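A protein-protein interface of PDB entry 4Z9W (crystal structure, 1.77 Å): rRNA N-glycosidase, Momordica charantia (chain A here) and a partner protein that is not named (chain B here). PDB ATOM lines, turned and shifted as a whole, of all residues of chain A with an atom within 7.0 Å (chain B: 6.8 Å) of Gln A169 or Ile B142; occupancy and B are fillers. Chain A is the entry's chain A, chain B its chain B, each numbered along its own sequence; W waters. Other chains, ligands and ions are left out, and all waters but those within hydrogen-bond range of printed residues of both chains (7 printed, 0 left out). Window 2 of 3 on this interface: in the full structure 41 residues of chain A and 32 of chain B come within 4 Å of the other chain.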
ATOM      1  N   TYR A  14      20.760  20.929  10.280  1.00  0.00           N
ATOM      2  CA  TYR A  14      20.489  20.562   8.882  1.00  0.00           C
ATOM      3  C   TYR A  14      19.194  21.207   8.425  1.00  0.00           C
ATOM      4  O   TYR A  14      19.148  21.881   7.375  1.00  0.00           O
ATOM      5  CB  TYR A  14      20.404  19.042   8.715  1.00  0.00           C
ATOM      6  CG  TYR A  14      19.968  18.639   7.336  1.00  0.00           C
ATOM      7  CD1 TYR A  14      20.851  18.746   6.245  1.00  0.00           C
ATOM      8  CD2 TYR A  14      18.681  18.188   7.102  1.00  0.00           C
ATOM      9  CE1 TYR A  14      20.447  18.397   4.960  1.00  0.00           C
ATOM     10  CE2 TYR A  14      18.267  17.818   5.827  1.00  0.00           C
ATOM     11  CZ  TYR A  14      19.160  17.935   4.757  1.00  0.00           C
ATOM     12  OH  TYR A  14      18.736  17.564   3.509  1.00  0.00           O
ATOM     13  N   LYS A  15      18.152  21.044   9.212  1.00  0.00           N
ATOM     14  CA  LYS A  15      16.886  21.666   8.852  1.00  0.00           C
ATOM     15  C   LYS A  15      16.992  23.188   8.683  1.00  0.00           C
ATOM     16  O   LYS A  15      16.448  23.748   7.724  1.00  0.00           O
ATOM     17  CB  LYS A  15      15.799  21.309   9.852  1.00  0.00           C
ATOM     18  CG  LYS A  15      14.447  21.843   9.457  1.00  0.00           C
ATOM     19  CD  LYS A  15      13.394  21.381  10.419  1.00  0.00           C
ATOM     20  CE  LYS A  15      12.025  21.419   9.808  1.00  0.00           C
ATOM     21  NZ  LYS A  15      11.821  20.433   8.699  1.00  0.00           N
ATOM     22  N   ARG A  22      16.714  27.599   0.936  1.00  0.00           N
ATOM     23  CA  ARG A  22      15.497  27.945   0.217  1.00  0.00           C
ATOM     24  C   ARG A  22      15.249  29.451   0.188  1.00  0.00           C
ATOM     25  O   ARG A  22      14.871  30.014  -0.846  1.00  0.00           O
ATOM     26  CB  ARG A  22      14.299  27.258   0.848  1.00  0.00           C
ATOM     27  CG  ARG A  22      14.277  25.761   0.597  1.00  0.00           C
ATOM     28  CD  ARG A  22      13.232  25.117   1.461  1.00  0.00           C
ATOM     29  NE  ARG A  22      13.198  23.665   1.272  1.00  0.00           N
ATOM     30  CZ  ARG A  22      12.818  22.796   2.203  1.00  0.00           C
ATOM     31  NH1 ARG A  22      12.354  23.205   3.383  1.00  0.00           N
ATOM     32  NH2 ARG A  22      12.860  21.483   1.938  1.00  0.00           N
ATOM     33  N   ALA A 161      16.905  18.067  -1.538  1.00  0.00           N
ATOM     34  CA  ALA A 161      16.304  18.343  -0.265  1.00  0.00           C
ATOM     35  C   ALA A 161      15.725  19.766  -0.184  1.00  0.00           C
ATOM     36  O   ALA A 161      14.614  19.949   0.315  1.00  0.00           O
ATOM     37  CB  ALA A 161      17.304  18.112   0.862  1.00  0.00           C
ATOM     38  N   PHE A 164      12.506  19.779  -2.300  1.00  0.00           N
ATOM     39  CA  PHE A 164      11.391  18.935  -1.827  1.00  0.00           C
ATOM     40  C   PHE A 164      11.452  18.632  -0.362  1.00  0.00           C
ATOM     41  O   PHE A 164      12.358  17.958   0.085  1.00  0.00           O
ATOM     42  CB  PHE A 164      11.378  17.602  -2.573  1.00  0.00           C
ATOM     43  CG  PHE A 164      11.123  17.726  -4.048  1.00  0.00           C
ATOM     44  CD1 PHE A 164       9.832  17.944  -4.520  1.00  0.00           C
ATOM     45  CD2 PHE A 164      12.166  17.634  -4.967  1.00  0.00           C
ATOM     46  CE1 PHE A 164       9.576  18.056  -5.887  1.00  0.00           C
ATOM     47  CE2 PHE A 164      11.903  17.726  -6.338  1.00  0.00           C
ATOM     48  CZ  PHE A 164      10.625  17.928  -6.784  1.00  0.00           C
ATOM     49  N   LYS A 165      10.431  19.061   0.385  1.00  0.00           N
ATOM     50  CA  LYS A 165      10.367  18.762   1.798  1.00  0.00           C
ATOM     51  C   LYS A 165      10.378  17.274   2.086  1.00  0.00           C
ATOM     52  O   LYS A 165      10.922  16.845   3.089  1.00  0.00           O
ATOM     53  CB  LYS A 165       9.144  19.413   2.449  1.00  0.00           C
ATOM     54  CG  LYS A 165       9.259  20.909   2.468  1.00  0.00           C
ATOM     55  CD  LYS A 165       7.947  21.561   2.892  1.00  0.00           C
ATOM     56  CE  LYS A 165       8.230  23.015   3.242  1.00  0.00           C
ATOM     57  NZ  LYS A 165       6.981  23.711   3.656  1.00  0.00           N
ATOM     58  N   PHE A 166       9.842  16.469   1.183  1.00  0.00           N
ATOM     59  CA  PHE A 166       9.880  15.027   1.361  1.00  0.00           C
ATOM     60  C   PHE A 166      11.311  14.504   1.472  1.00  0.00           C
ATOM     61  O   PHE A 166      11.646  13.690   2.344  1.00  0.00           O
ATOM     62  CB  PHE A 166       9.101  14.356   0.209  1.00  0.00           C
ATOM     63  CG  PHE A 166       9.156  12.854   0.224  1.00  0.00           C
ATOM     64  CD1 PHE A 166      10.213  12.166  -0.359  1.00  0.00           C
ATOM     65  CD2 PHE A 166       8.164  12.121   0.867  1.00  0.00           C
ATOM     66  CE1 PHE A 166      10.262  10.784  -0.331  1.00  0.00           C
ATOM     67  CE2 PHE A 166       8.233  10.724   0.913  1.00  0.00           C
ATOM     68  CZ  PHE A 166       9.267  10.063   0.296  1.00  0.00           C
ATOM     69  N   ILE A 167      12.176  15.004   0.607  1.00  0.00           N
ATOM     70  CA  ILE A 167      13.539  14.590   0.572  1.00  0.00           C
ATOM     71  C   ILE A 167      14.281  15.144   1.806  1.00  0.00           C
ATOM     72  O   ILE A 167      14.999  14.414   2.446  1.00  0.00           O
ATOM     73  CB  ILE A 167      14.214  14.995  -0.733  1.00  0.00           C
ATOM     74  CG1 ILE A 167      13.510  14.300  -1.910  1.00  0.00           C
ATOM     75  CG2 ILE A 167      15.706  14.670  -0.668  1.00  0.00           C
ATOM     76  CD1 ILE A 167      14.093  14.677  -3.263  1.00  0.00           C
ATOM     77  N   GLU A 168      14.039  16.405   2.139  1.00  0.00           N
ATOM     78  CA  GLU A 168      14.531  16.963   3.407  1.00  0.00           C
ATOM     79  C   GLU A 168      14.174  16.030   4.587  1.00  0.00           C
ATOM     80  O   GLU A 168      15.047  15.713   5.431  1.00  0.00           O
ATOM     81  CB  GLU A 168      13.957  18.361   3.598  1.00  0.00           C
ATOM     82  CG  GLU A 168      14.318  19.006   4.924  1.00  0.00           C
ATOM     83  CD  GLU A 168      13.360  20.118   5.343  1.00  0.00           C
ATOM     84  OE1 GLU A 168      12.517  20.559   4.552  1.00  0.00           O
ATOM     85  OE2 GLU A 168      13.473  20.572   6.510  1.00  0.00           O
ATOM     86  N   GLN A 169      12.916  15.616   4.679  1.00  0.00           N
ATOM     87  CA  GLN A 169      12.492  14.738   5.765  1.00  0.00           C
ATOM     88  C   GLN A 169      13.180  13.353   5.760  1.00  0.00           C
ATOM     89  O   GLN A 169      13.509  12.827   6.835  1.00  0.00           O
ATOM     90  CB  GLN A 169      10.968  14.577   5.819  1.00  0.00           C
ATOM     91  CG  GLN A 169      10.227  15.884   6.096  1.00  0.00           C
ATOM     92  CD  GLN A 169      10.589  16.499   7.445  1.00  0.00           C
ATOM     93  OE1 GLN A 169      10.840  15.794   8.441  1.00  0.00           O
ATOM     94  NE2 GLN A 169      10.644  17.812   7.474  1.00  0.00           N
ATOM     95  N   LYS A 170      13.408  12.790   4.577  1.00  0.00           N
ATOM     96  CA  LYS A 170      14.180  11.552   4.453  1.00  0.00           C
ATOM     97  C   LYS A 170      15.544  11.707   5.062  1.00  0.00           C
ATOM     98  O   LYS A 170      16.016  10.841   5.805  1.00  0.00           O
ATOM     99  CB  LYS A 170      14.399  11.153   2.993  1.00  0.00           C
ATOM    100  CG  LYS A 170      13.192  10.662   2.253  1.00  0.00           C
ATOM    101  CD  LYS A 170      12.839   9.219   2.580  1.00  0.00           C
ATOM    102  CE  LYS A 170      13.754   8.192   1.935  1.00  0.00           C
ATOM    103  NZ  LYS A 170      13.309   6.832   2.335  1.00  0.00           N
ATOM    104  N   VAL A 171      16.212  12.806   4.732  1.00  0.00           N
ATOM    105  CA  VAL A 171      17.530  13.065   5.249  1.00  0.00           C
ATOM    106  C   VAL A 171      17.446  13.273   6.782  1.00  0.00           C
ATOM    107  O   VAL A 171      18.261  12.734   7.537  1.00  0.00           O
ATOM    108  CB  VAL A 171      18.199  14.259   4.544  1.00  0.00           C
ATOM    109  CG1 VAL A 171      19.543  14.557   5.162  1.00  0.00           C
ATOM    110  CG2 VAL A 171      18.380  13.990   3.049  1.00  0.00           C
ATOM    111  N   ILE A 172      16.448  14.030   7.243  1.00  0.00           N
ATOM    112  CA  ILE A 172      16.262  14.181   8.694  1.00  0.00           C
ATOM    113  C   ILE A 172      16.101  12.821   9.408  1.00  0.00           C
ATOM    114  O   ILE A 172      16.751  12.617  10.449  1.00  0.00           O
ATOM    115  CB  ILE A 172      15.094  15.151   9.037  1.00  0.00           C
ATOM    116  CG1 ILE A 172      15.501  16.588   8.716  1.00  0.00           C
ATOM    117  CG2 ILE A 172      14.701  15.069  10.530  1.00  0.00           C
ATOM    118  CD1 ILE A 172      14.340  17.571   8.648  1.00  0.00           C
ATOM    119  N   HIS A 173      15.252  11.928   8.874  1.00  0.00           N
ATOM    120  CA  HIS A 173      15.083  10.557   9.413  1.00  0.00           C
ATOM    121  C   HIS A 173      16.478   9.880   9.538  1.00  0.00           C
ATOM    122  O   HIS A 173      16.840   9.320  10.595  1.00  0.00           O
ATOM    123  CB  HIS A 173      14.110   9.720   8.563  1.00  0.00           C
ATOM    124  CG  HIS A 173      12.641  10.025   8.767  1.00  0.00           C
ATOM    125  ND1 HIS A 173      11.737  10.069   7.720  1.00  0.00           N
ATOM    126  CD2 HIS A 173      11.909  10.249   9.891  1.00  0.00           C
ATOM    127  CE1 HIS A 173      10.527  10.334   8.183  1.00  0.00           C
ATOM    128  NE2 HIS A 173      10.599  10.437   9.500  1.00  0.00           N
ATOM    129  N   SER A 174      17.277  10.017   8.484  1.00  0.00           N
ATOM    130  CA  SER A 174      18.597   9.429   8.418  1.00  0.00           C
ATOM    131  C   SER A 174      19.597   9.979   9.458  1.00  0.00           C
ATOM    132  O   SER A 174      20.389   9.206  10.033  1.00  0.00           O
ATOM    133  CB  SER A 174      19.164   9.617   7.020  1.00  0.00           C
ATOM    134  OG  SER A 174      20.383   8.938   6.913  1.00  0.00           O
ATOM    135  N   ILE A 175      19.576  11.291   9.681  1.00  0.00           N
ATOM    136  CA  ILE A 175      20.471  11.944  10.664  1.00  0.00           C
ATOM    137  C   ILE A 175      20.065  11.577  12.083  1.00  0.00           C
ATOM    138  O   ILE A 175      20.926  11.289  12.937  1.00  0.00           O
ATOM    139  CB  ILE A 175      20.413  13.480  10.587  1.00  0.00           C
ATOM    140  CG1 ILE A 175      20.986  13.980   9.265  1.00  0.00           C
ATOM    141  CG2 ILE A 175      21.198  14.126  11.749  1.00  0.00           C
ATOM    142  CD1 ILE A 175      20.608  15.420   8.963  1.00  0.00           C
ATOM    143  N   MET A 176      18.764  11.627  12.350  1.00  0.00           N
ATOM    144  CA  MET A 176      18.277  11.378  13.695  1.00  0.00           C
ATOM    145  C   MET A 176      18.683   9.999  14.157  1.00  0.00           C
ATOM    146  O   MET A 176      19.110   9.840  15.305  1.00  0.00           O
ATOM    147  CB  MET A 176      16.757  11.561  13.785  1.00  0.00           C
ATOM    148  CG  MET A 176      16.372  13.042  13.731  1.00  0.00           C
ATOM    149  SD  MET A 176      14.596  13.441  13.774  1.00  0.00           S
ATOM    150  CE  MET A 176      14.249  13.256  15.532  1.00  0.00           C
ATOM    151  N   THR B 140       2.107  10.167   6.758  1.00  0.00           N
ATOM    152  CA  THR B 140       2.361  10.661   8.112  1.00  0.00           C
ATOM    153  C   THR B 140       2.381  12.164   7.968  1.00  0.00           C
ATOM    154  O   THR B 140       2.466  12.699   6.848  1.00  0.00           O
ATOM    155  CB  THR B 140       3.665  10.122   8.717  1.00  0.00           C
ATOM    156  OG1 THR B 140       4.785  10.545   7.926  1.00  0.00           O
ATOM    157  CG2 THR B 140       3.652   8.617   8.778  1.00  0.00           C
ATOM    158  N   ILE B 141       2.253  12.839   9.104  1.00  0.00           N
ATOM    159  CA  ILE B 141       2.166  14.274   9.141  1.00  0.00           C
ATOM    160  C   ILE B 141       3.177  14.645  10.203  1.00  0.00           C
ATOM    161  O   ILE B 141       3.006  14.279  11.367  1.00  0.00           O
ATOM    162  CB  ILE B 141       0.761  14.781   9.516  1.00  0.00           C
ATOM    163  CG1 ILE B 141      -0.225  14.499   8.389  1.00  0.00           C
ATOM    164  CG2 ILE B 141       0.794  16.280   9.767  1.00  0.00           C
ATOM    165  CD1 ILE B 141      -1.662  14.751   8.756  1.00  0.00           C
ATOM    166  N   ILE B 142       4.215  15.381   9.791  1.00  0.00           N
ATOM    167  CA  ILE B 142       5.362  15.646  10.634  1.00  0.00           C
ATOM    168  C   ILE B 142       5.312  17.085  11.083  1.00  0.00           C
ATOM    169  O   ILE B 142       5.057  17.973  10.290  1.00  0.00           O
ATOM    170  CB  ILE B 142       6.679  15.398   9.887  1.00  0.00           C
ATOM    171  CG1 ILE B 142       6.707  13.951   9.373  1.00  0.00           C
ATOM    172  CG2 ILE B 142       7.877  15.658  10.792  1.00  0.00           C
ATOM    173  CD1 ILE B 142       7.986  13.601   8.653  1.00  0.00           C
ATOM    174  N   GLY B 143       5.581  17.306  12.362  1.00  0.00           N
ATOM    175  CA  GLY B 143       5.466  18.646  12.940  1.00  0.00           C
ATOM    176  C   GLY B 143       6.651  18.935  13.831  1.00  0.00           C
ATOM    177  O   GLY B 143       7.781  18.491  13.562  1.00  0.00           O
ATOM    178  N   LEU B 144       6.402  19.703  14.894  1.00  0.00           N
ATOM    179  CA  LEU B 144       7.472  20.175  15.768  1.00  0.00           C
ATOM    180  C   LEU B 144       8.334  19.057  16.354  1.00  0.00           C
ATOM    181  O   LEU B 144       7.866  17.970  16.612  1.00  0.00           O
ATOM    182  CB  LEU B 144       6.895  21.046  16.877  1.00  0.00           C
ATOM    183  CG  LEU B 144       7.840  21.922  17.702  1.00  0.00           C
ATOM    184  CD1 LEU B 144       8.523  22.979  16.835  1.00  0.00           C
ATOM    185  CD2 LEU B 144       6.990  22.584  18.774  1.00  0.00           C
ATOM    186  N   ARG B 145       9.608  19.357  16.557  1.00  0.00           N
ATOM    187  CA  ARG B 145      10.637  18.400  17.039  1.00  0.00           C
ATOM    188  C   ARG B 145      10.734  17.164  16.155  1.00  0.00           C
ATOM    189  O   ARG B 145      11.112  16.102  16.609  1.00  0.00           O
ATOM    190  CB  ARG B 145      10.402  18.022  18.506  1.00  0.00           C
ATOM    191  CG  ARG B 145      10.166  19.228  19.439  1.00  0.00           C
ATOM    192  CD  ARG B 145      11.200  20.372  19.314  1.00  0.00           C
ATOM    193  NE  ARG B 145      12.603  19.903  19.455  1.00  0.00           N
ATOM    194  CZ  ARG B 145      13.627  20.103  18.595  1.00  0.00           C
ATOM    195  NH1 ARG B 145      13.492  20.788  17.463  1.00  0.00           N
ATOM    196  NH2 ARG B 145      14.827  19.605  18.882  1.00  0.00           N
ATOM    197  N   HIS B 146      10.397  17.338  14.875  1.00  0.00           N
ATOM    198  CA  HIS B 146      10.446  16.260  13.885  1.00  0.00           C
ATOM    199  C   HIS B 146       9.549  15.093  14.261  1.00  0.00           C
ATOM    200  O   HIS B 146       9.822  13.957  13.899  1.00  0.00           O
ATOM    201  CB  HIS B 146      11.898  15.778  13.655  1.00  0.00           C
ATOM    202  CG  HIS B 146      12.926  16.864  13.736  1.00  0.00           C
ATOM    203  ND1 HIS B 146      13.238  17.676  12.669  1.00  0.00           N
ATOM    204  CD2 HIS B 146      13.719  17.266  14.765  1.00  0.00           C
ATOM    205  CE1 HIS B 146      14.190  18.518  13.024  1.00  0.00           C
ATOM    206  NE2 HIS B 146      14.495  18.299  14.296  1.00  0.00           N
ATOM    207  N   MET B 147       8.455  15.368  14.973  1.00  0.00           N
ATOM    208  CA  MET B 147       7.582  14.328  15.456  1.00  0.00           C
ATOM    209  C   MET B 147       6.415  14.125  14.522  1.00  0.00           C
ATOM    210  O   MET B 147       6.195  14.938  13.622  1.00  0.00           O
ATOM    211  CB  MET B 147       7.118  14.652  16.887  1.00  0.00           C
ATOM    212  CG  MET B 147       8.147  14.330  17.940  1.00  0.00           C
ATOM    213  SD  MET B 147       7.400  14.630  19.580  1.00  0.00           S
ATOM    214  CE  MET B 147       8.728  14.062  20.635  1.00  0.00           C
ATOM    215  N   CYS B 148       5.678  13.031  14.750  1.00  0.00           N
ATOM    216  CA  CYS B 148       4.538  12.615  13.939  1.00  0.00           C
ATOM    217  C   CYS B 148       3.232  12.824  14.707  1.00  0.00           C
ATOM    218  O   CYS B 148       3.157  12.460  15.870  1.00  0.00           O
ATOM    219  CB  CYS B 148       4.661  11.098  13.561  1.00  0.00           C
ATOM    220  SG  CYS B 148       5.788  10.791  12.164  1.00  0.00           S
ATOM    221  N   LEU B 149       2.201  13.308  14.031  1.00  0.00           N
ATOM    222  CA  LEU B 149       0.861  13.360  14.640  1.00  0.00           C
ATOM    223  C   LEU B 149       0.365  11.922  14.806  1.00  0.00           C
ATOM    224  O   LEU B 149       0.555  11.082  13.923  1.00  0.00           O
ATOM    225  CB  LEU B 149      -0.145  14.120  13.791  1.00  0.00           C
ATOM    226  CG  LEU B 149      -0.174  15.634  13.803  1.00  0.00           C
ATOM    227  CD1 LEU B 149      -1.240  16.149  12.871  1.00  0.00           C
ATOM    228  CD2 LEU B 149      -0.402  16.160  15.209  1.00  0.00           C
ATOM    229  N   LEU B 160       1.555  15.081  19.022  1.00  0.00           N
ATOM    230  CA  LEU B 160       2.835  14.649  18.469  1.00  0.00           C
ATOM    231  C   LEU B 160       3.529  13.588  19.299  1.00  0.00           C
ATOM    232  O   LEU B 160       3.631  13.698  20.536  1.00  0.00           O
ATOM    233  CB  LEU B 160       3.770  15.847  18.217  1.00  0.00           C
ATOM    234  CG  LEU B 160       3.346  16.780  17.082  1.00  0.00           C
ATOM    235  CD1 LEU B 160       3.988  18.165  17.246  1.00  0.00           C
ATOM    236  CD2 LEU B 160       3.683  16.216  15.705  1.00  0.00           C
ATOM    237  N   CYS B 163       8.194   9.571  15.632  1.00  0.00           N
ATOM    238  CA  CYS B 163       7.815   8.790  14.464  1.00  0.00           C
ATOM    239  C   CYS B 163       8.328   7.361  14.599  1.00  0.00           C
ATOM    240  O   CYS B 163       9.495   7.144  14.939  1.00  0.00           O
ATOM    241  CB  CYS B 163       8.381   9.416  13.181  1.00  0.00           C
ATOM    242  SG  CYS B 163       7.757  11.089  12.836  1.00  0.00           S
ATOM    243  N   ILE B 222      -0.893  24.089   8.245  1.00  0.00           N
ATOM    244  CA  ILE B 222      -2.124  23.348   8.030  1.00  0.00           C
ATOM    245  C   ILE B 222      -3.238  24.320   8.460  1.00  0.00           C
ATOM    246  O   ILE B 222      -3.453  24.558   9.643  1.00  0.00           O
ATOM    247  CB  ILE B 222      -2.177  22.031   8.786  1.00  0.00           C
ATOM    248  CG1 ILE B 222      -0.913  21.210   8.517  1.00  0.00           C
ATOM    249  CG2 ILE B 222      -3.410  21.228   8.345  1.00  0.00           C
ATOM    250  CD1 ILE B 222      -0.832  19.879   9.237  1.00  0.00           C
ATOM    251  N   GLN B 256       4.587  24.811  11.805  1.00  0.00           N
ATOM    252  CA  GLN B 256       5.160  24.198  10.613  1.00  0.00           C
ATOM    253  C   GLN B 256       4.919  22.712  10.613  1.00  0.00           C
ATOM    254  O   GLN B 256       5.202  22.022  11.589  1.00  0.00           O
ATOM    255  CB  GLN B 256       6.654  24.512  10.491  1.00  0.00           C
ATOM    256  CG  GLN B 256       6.895  25.956  10.102  1.00  0.00           C
ATOM    257  CD  GLN B 256       6.481  26.272   8.673  1.00  0.00           C
ATOM    258  OE1 GLN B 256       6.909  25.622   7.730  1.00  0.00           O
ATOM    259  NE2 GLN B 256       5.637  27.259   8.515  1.00  0.00           N
ATOM    260  N   TRP B 257       4.438  22.225   9.476  1.00  0.00           N
ATOM    261  CA  TRP B 257       4.182  20.826   9.279  1.00  0.00           C
ATOM    262  C   TRP B 257       4.569  20.426   7.868  1.00  0.00           C
ATOM    263  O   TRP B 257       4.617  21.264   6.979  1.00  0.00           O
ATOM    264  CB  TRP B 257       2.697  20.536   9.429  1.00  0.00           C
ATOM    265  CG  TRP B 257       2.096  21.059  10.664  1.00  0.00           C
ATOM    266  CD1 TRP B 257       1.687  22.330  10.892  1.00  0.00           C
ATOM    267  CD2 TRP B 257       1.891  20.341  11.877  1.00  0.00           C
ATOM    268  NE1 TRP B 257       1.195  22.445  12.179  1.00  0.00           N
ATOM    269  CE2 TRP B 257       1.324  21.240  12.805  1.00  0.00           C
ATOM    270  CE3 TRP B 257       2.103  19.014  12.263  1.00  0.00           C
ATOM    271  CZ2 TRP B 257       0.952  20.853  14.104  1.00  0.00           C
ATOM    272  CZ3 TRP B 257       1.762  18.633  13.579  1.00  0.00           C
ATOM    273  CH2 TRP B 257       1.194  19.564  14.479  1.00  0.00           C
ATOM    274  N   THR B 258       4.801  19.144   7.659  1.00  0.00           N
ATOM    275  CA  THR B 258       4.720  18.661   6.291  1.00  0.00           C
ATOM    276  C   THR B 258       4.216  17.211   6.211  1.00  0.00           C
ATOM    277  O   THR B 258       3.822  16.615   7.227  1.00  0.00           O
ATOM    278  CB  THR B 258       6.066  18.860   5.580  1.00  0.00           C
ATOM    279  OG1 THR B 258       5.874  18.684   4.144  1.00  0.00           O
ATOM    280  CG2 THR B 258       7.117  17.914   6.192  1.00  0.00           C
ATOM    281  N   VAL B 259       4.174  16.679   5.008  1.00  0.00           N
ATOM    282  CA  VAL B 259       3.639  15.342   4.772  1.00  0.00           C
ATOM    283  C   VAL B 259       4.789  14.431   4.405  1.00  0.00           C
ATOM    284  O   VAL B 259       5.732  14.838   3.684  1.00  0.00           O
ATOM    285  CB  VAL B 259       2.534  15.317   3.685  1.00  0.00           C
ATOM    286  CG1 VAL B 259       1.361  16.158   4.144  1.00  0.00           C
ATOM    287  CG2 VAL B 259       3.043  15.787   2.334  1.00  0.00           C
ATOM    288  N   PHE B 260       4.760  13.236   4.954  1.00  0.00           N
ATOM    289  CA  PHE B 260       5.739  12.237   4.599  1.00  0.00           C
ATOM    290  C   PHE B 260       4.986  10.956   4.283  1.00  0.00           C
ATOM    291  O   PHE B 260       4.551  10.225   5.187  1.00  0.00           O
ATOM    292  CB  PHE B 260       6.774  11.991   5.665  1.00  0.00           C
ATOM    293  CG  PHE B 260       7.830  11.065   5.191  1.00  0.00           C
ATOM    294  CD1 PHE B 260       8.832  11.532   4.357  1.00  0.00           C
ATOM    295  CD2 PHE B 260       7.752   9.703   5.453  1.00  0.00           C
ATOM    296  CE1 PHE B 260       9.782  10.662   3.872  1.00  0.00           C
ATOM    297  CE2 PHE B 260       8.683   8.821   4.938  1.00  0.00           C
ATOM    298  CZ  PHE B 260       9.700   9.305   4.149  1.00  0.00           C
HETATM  299  O   HOH W   1       6.526  16.649   1.684  1.00  0.00           O
HETATM  300  O   HOH W   2      11.471  17.848  10.665  1.00  0.00           O
HETATM  301  O   HOH W   3       7.795  26.438   5.037  1.00  0.00           O
HETATM  302  O   HOH W   4       6.598  23.066   6.608  1.00  0.00           O
HETATM  303  O   HOH W   5       7.135  10.105   9.136  1.00  0.00           O
HETATM  304  O   HOH W   6       4.408  21.793   4.114  1.00  0.00           O
HETATM  305  O   HOH W   7      11.004  12.640  11.711  1.00  0.00           O
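The side-chain carboxylate of Glu A168 lies within salt-bridge range of the side-chain amino group of Lys A15 (2.7 Å).
The side-chain amino group (NZ) of Lys A15 lies close to the side-chain amide nitrogen (NE2) of Gln A169, at 3.1 Å.
O of Gln A169 is in hydrogen-bond range of ND1 of His A173 (3.4 Å).
The side-chain hydroxyl (OG1) of Thr B140 is in hydrogen-bond range of the backbone carbonyl oxygen (O) of Phe B260, 2.8 Å away.
The backbone NH of Ile B142 is in hydrogen-bond range of the backbone carbonyl oxygen of Thr B258 (2.9 Å).
The side-chain sulfur (SG) of Cys B148 forms a disulfide with the side-chain sulfur (SG) of Cys B163, at 2.1 Å.
Among the printed residues, pairs that only touch across the chains: Phe A166 with Phe B260, Lys A170 with Phe B260, Met A176 with His B146, Gln A169 with Ile B142, Ile A172 with His B146, Gln A169 with Thr B258, Lys A165 with Thr B258, His A173 with Phe B260, Lys A15 with His B146 and Gln A169 with Phe B260.
Of the printed residues of chain B, Lys A15 touches His B146.
Of the printed residues of chain B, Gln A169 touches Ile B142 (3.6 Å), Thr B258 (3.7 Å) and Phe B260 (3.996 Å).
Printed residues of chain B within 4 Å of His A173: Phe B260 (3.9 Å).
Of the printed residues of chain B, Met A176 touches His B146.
Ile B142 touches just one residue of chain A: Gln A169 (3.6 Å).
Met B147 touches none of the printed residues of chain A.
Printed residues of chain A within 4 Å of Thr B258: Lys A165 and Gln A169.
The nearest printed residue of chain B that does not touch Gln A169 is Val B259 (5.2 Å).
The nearest residue of chain A that does not touch Ile B142 is His A173 (4.2 Å).
The nearest printed residue of chain B that does not touch His A173 is Ile B142 (4.2 Å).
Hydrophobic or aromatic side chains of chain A that line the printed part of chain B: Phe A166, Ile A172, His A173 and Met A176.
Of the 18 printed residues of chain B, 4 touch a printed residue of chain A.
Hydrophobic or aromatic side chains of chain B that line the printed part of chain A: Ile B142, His B146 and Phe B260.
Water W2 lies within hydrogen-bond range of ND1 of His B146 (2.7 Å), OE1 of Gln A169 (3.1 Å) and NZ of Lys A15 (3.3 Å).
Water W5 lies within hydrogen-bond range of OG1 of Thr B140 (2.7 Å), SG of Cys B148 (3.4 Å) and NE2 of His A173 (3.5 Å).
Water W4 lies within hydrogen-bond range of the backbone carbonyl oxygen (O) of Trp B257 (2.7 Å), the side-chain amide oxygen (OE1) of Gln B256 (2.8 Å) and the side-chain amino group (NZ) of Lys A165 (3.0 Å).
Water W1 lies within hydrogen-bond range of the backbone carbonyl oxygen of Val B259 (2.8 Å), the side-chain hydroxyl of Thr B258 (3.3 Å) and the backbone NH of Phe A166 (3.4 Å).
Water W7 lies within hydrogen-bond range of the backbone carbonyl oxygen of His B146 (2.8 Å), a ring nitrogen (NE2) of His A173 (3.1 Å) and the side-chain sulfur of Cys B163 (3.8 Å).
Water W6 lies within hydrogen-bond range of the backbone carbonyl oxygen (O) of Trp B257 (2.9 Å), the side-chain amino group (NZ) of Lys A165 (3.2 Å) and the side-chain hydroxyl (OG1) of Thr B258 (3.4 Å).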
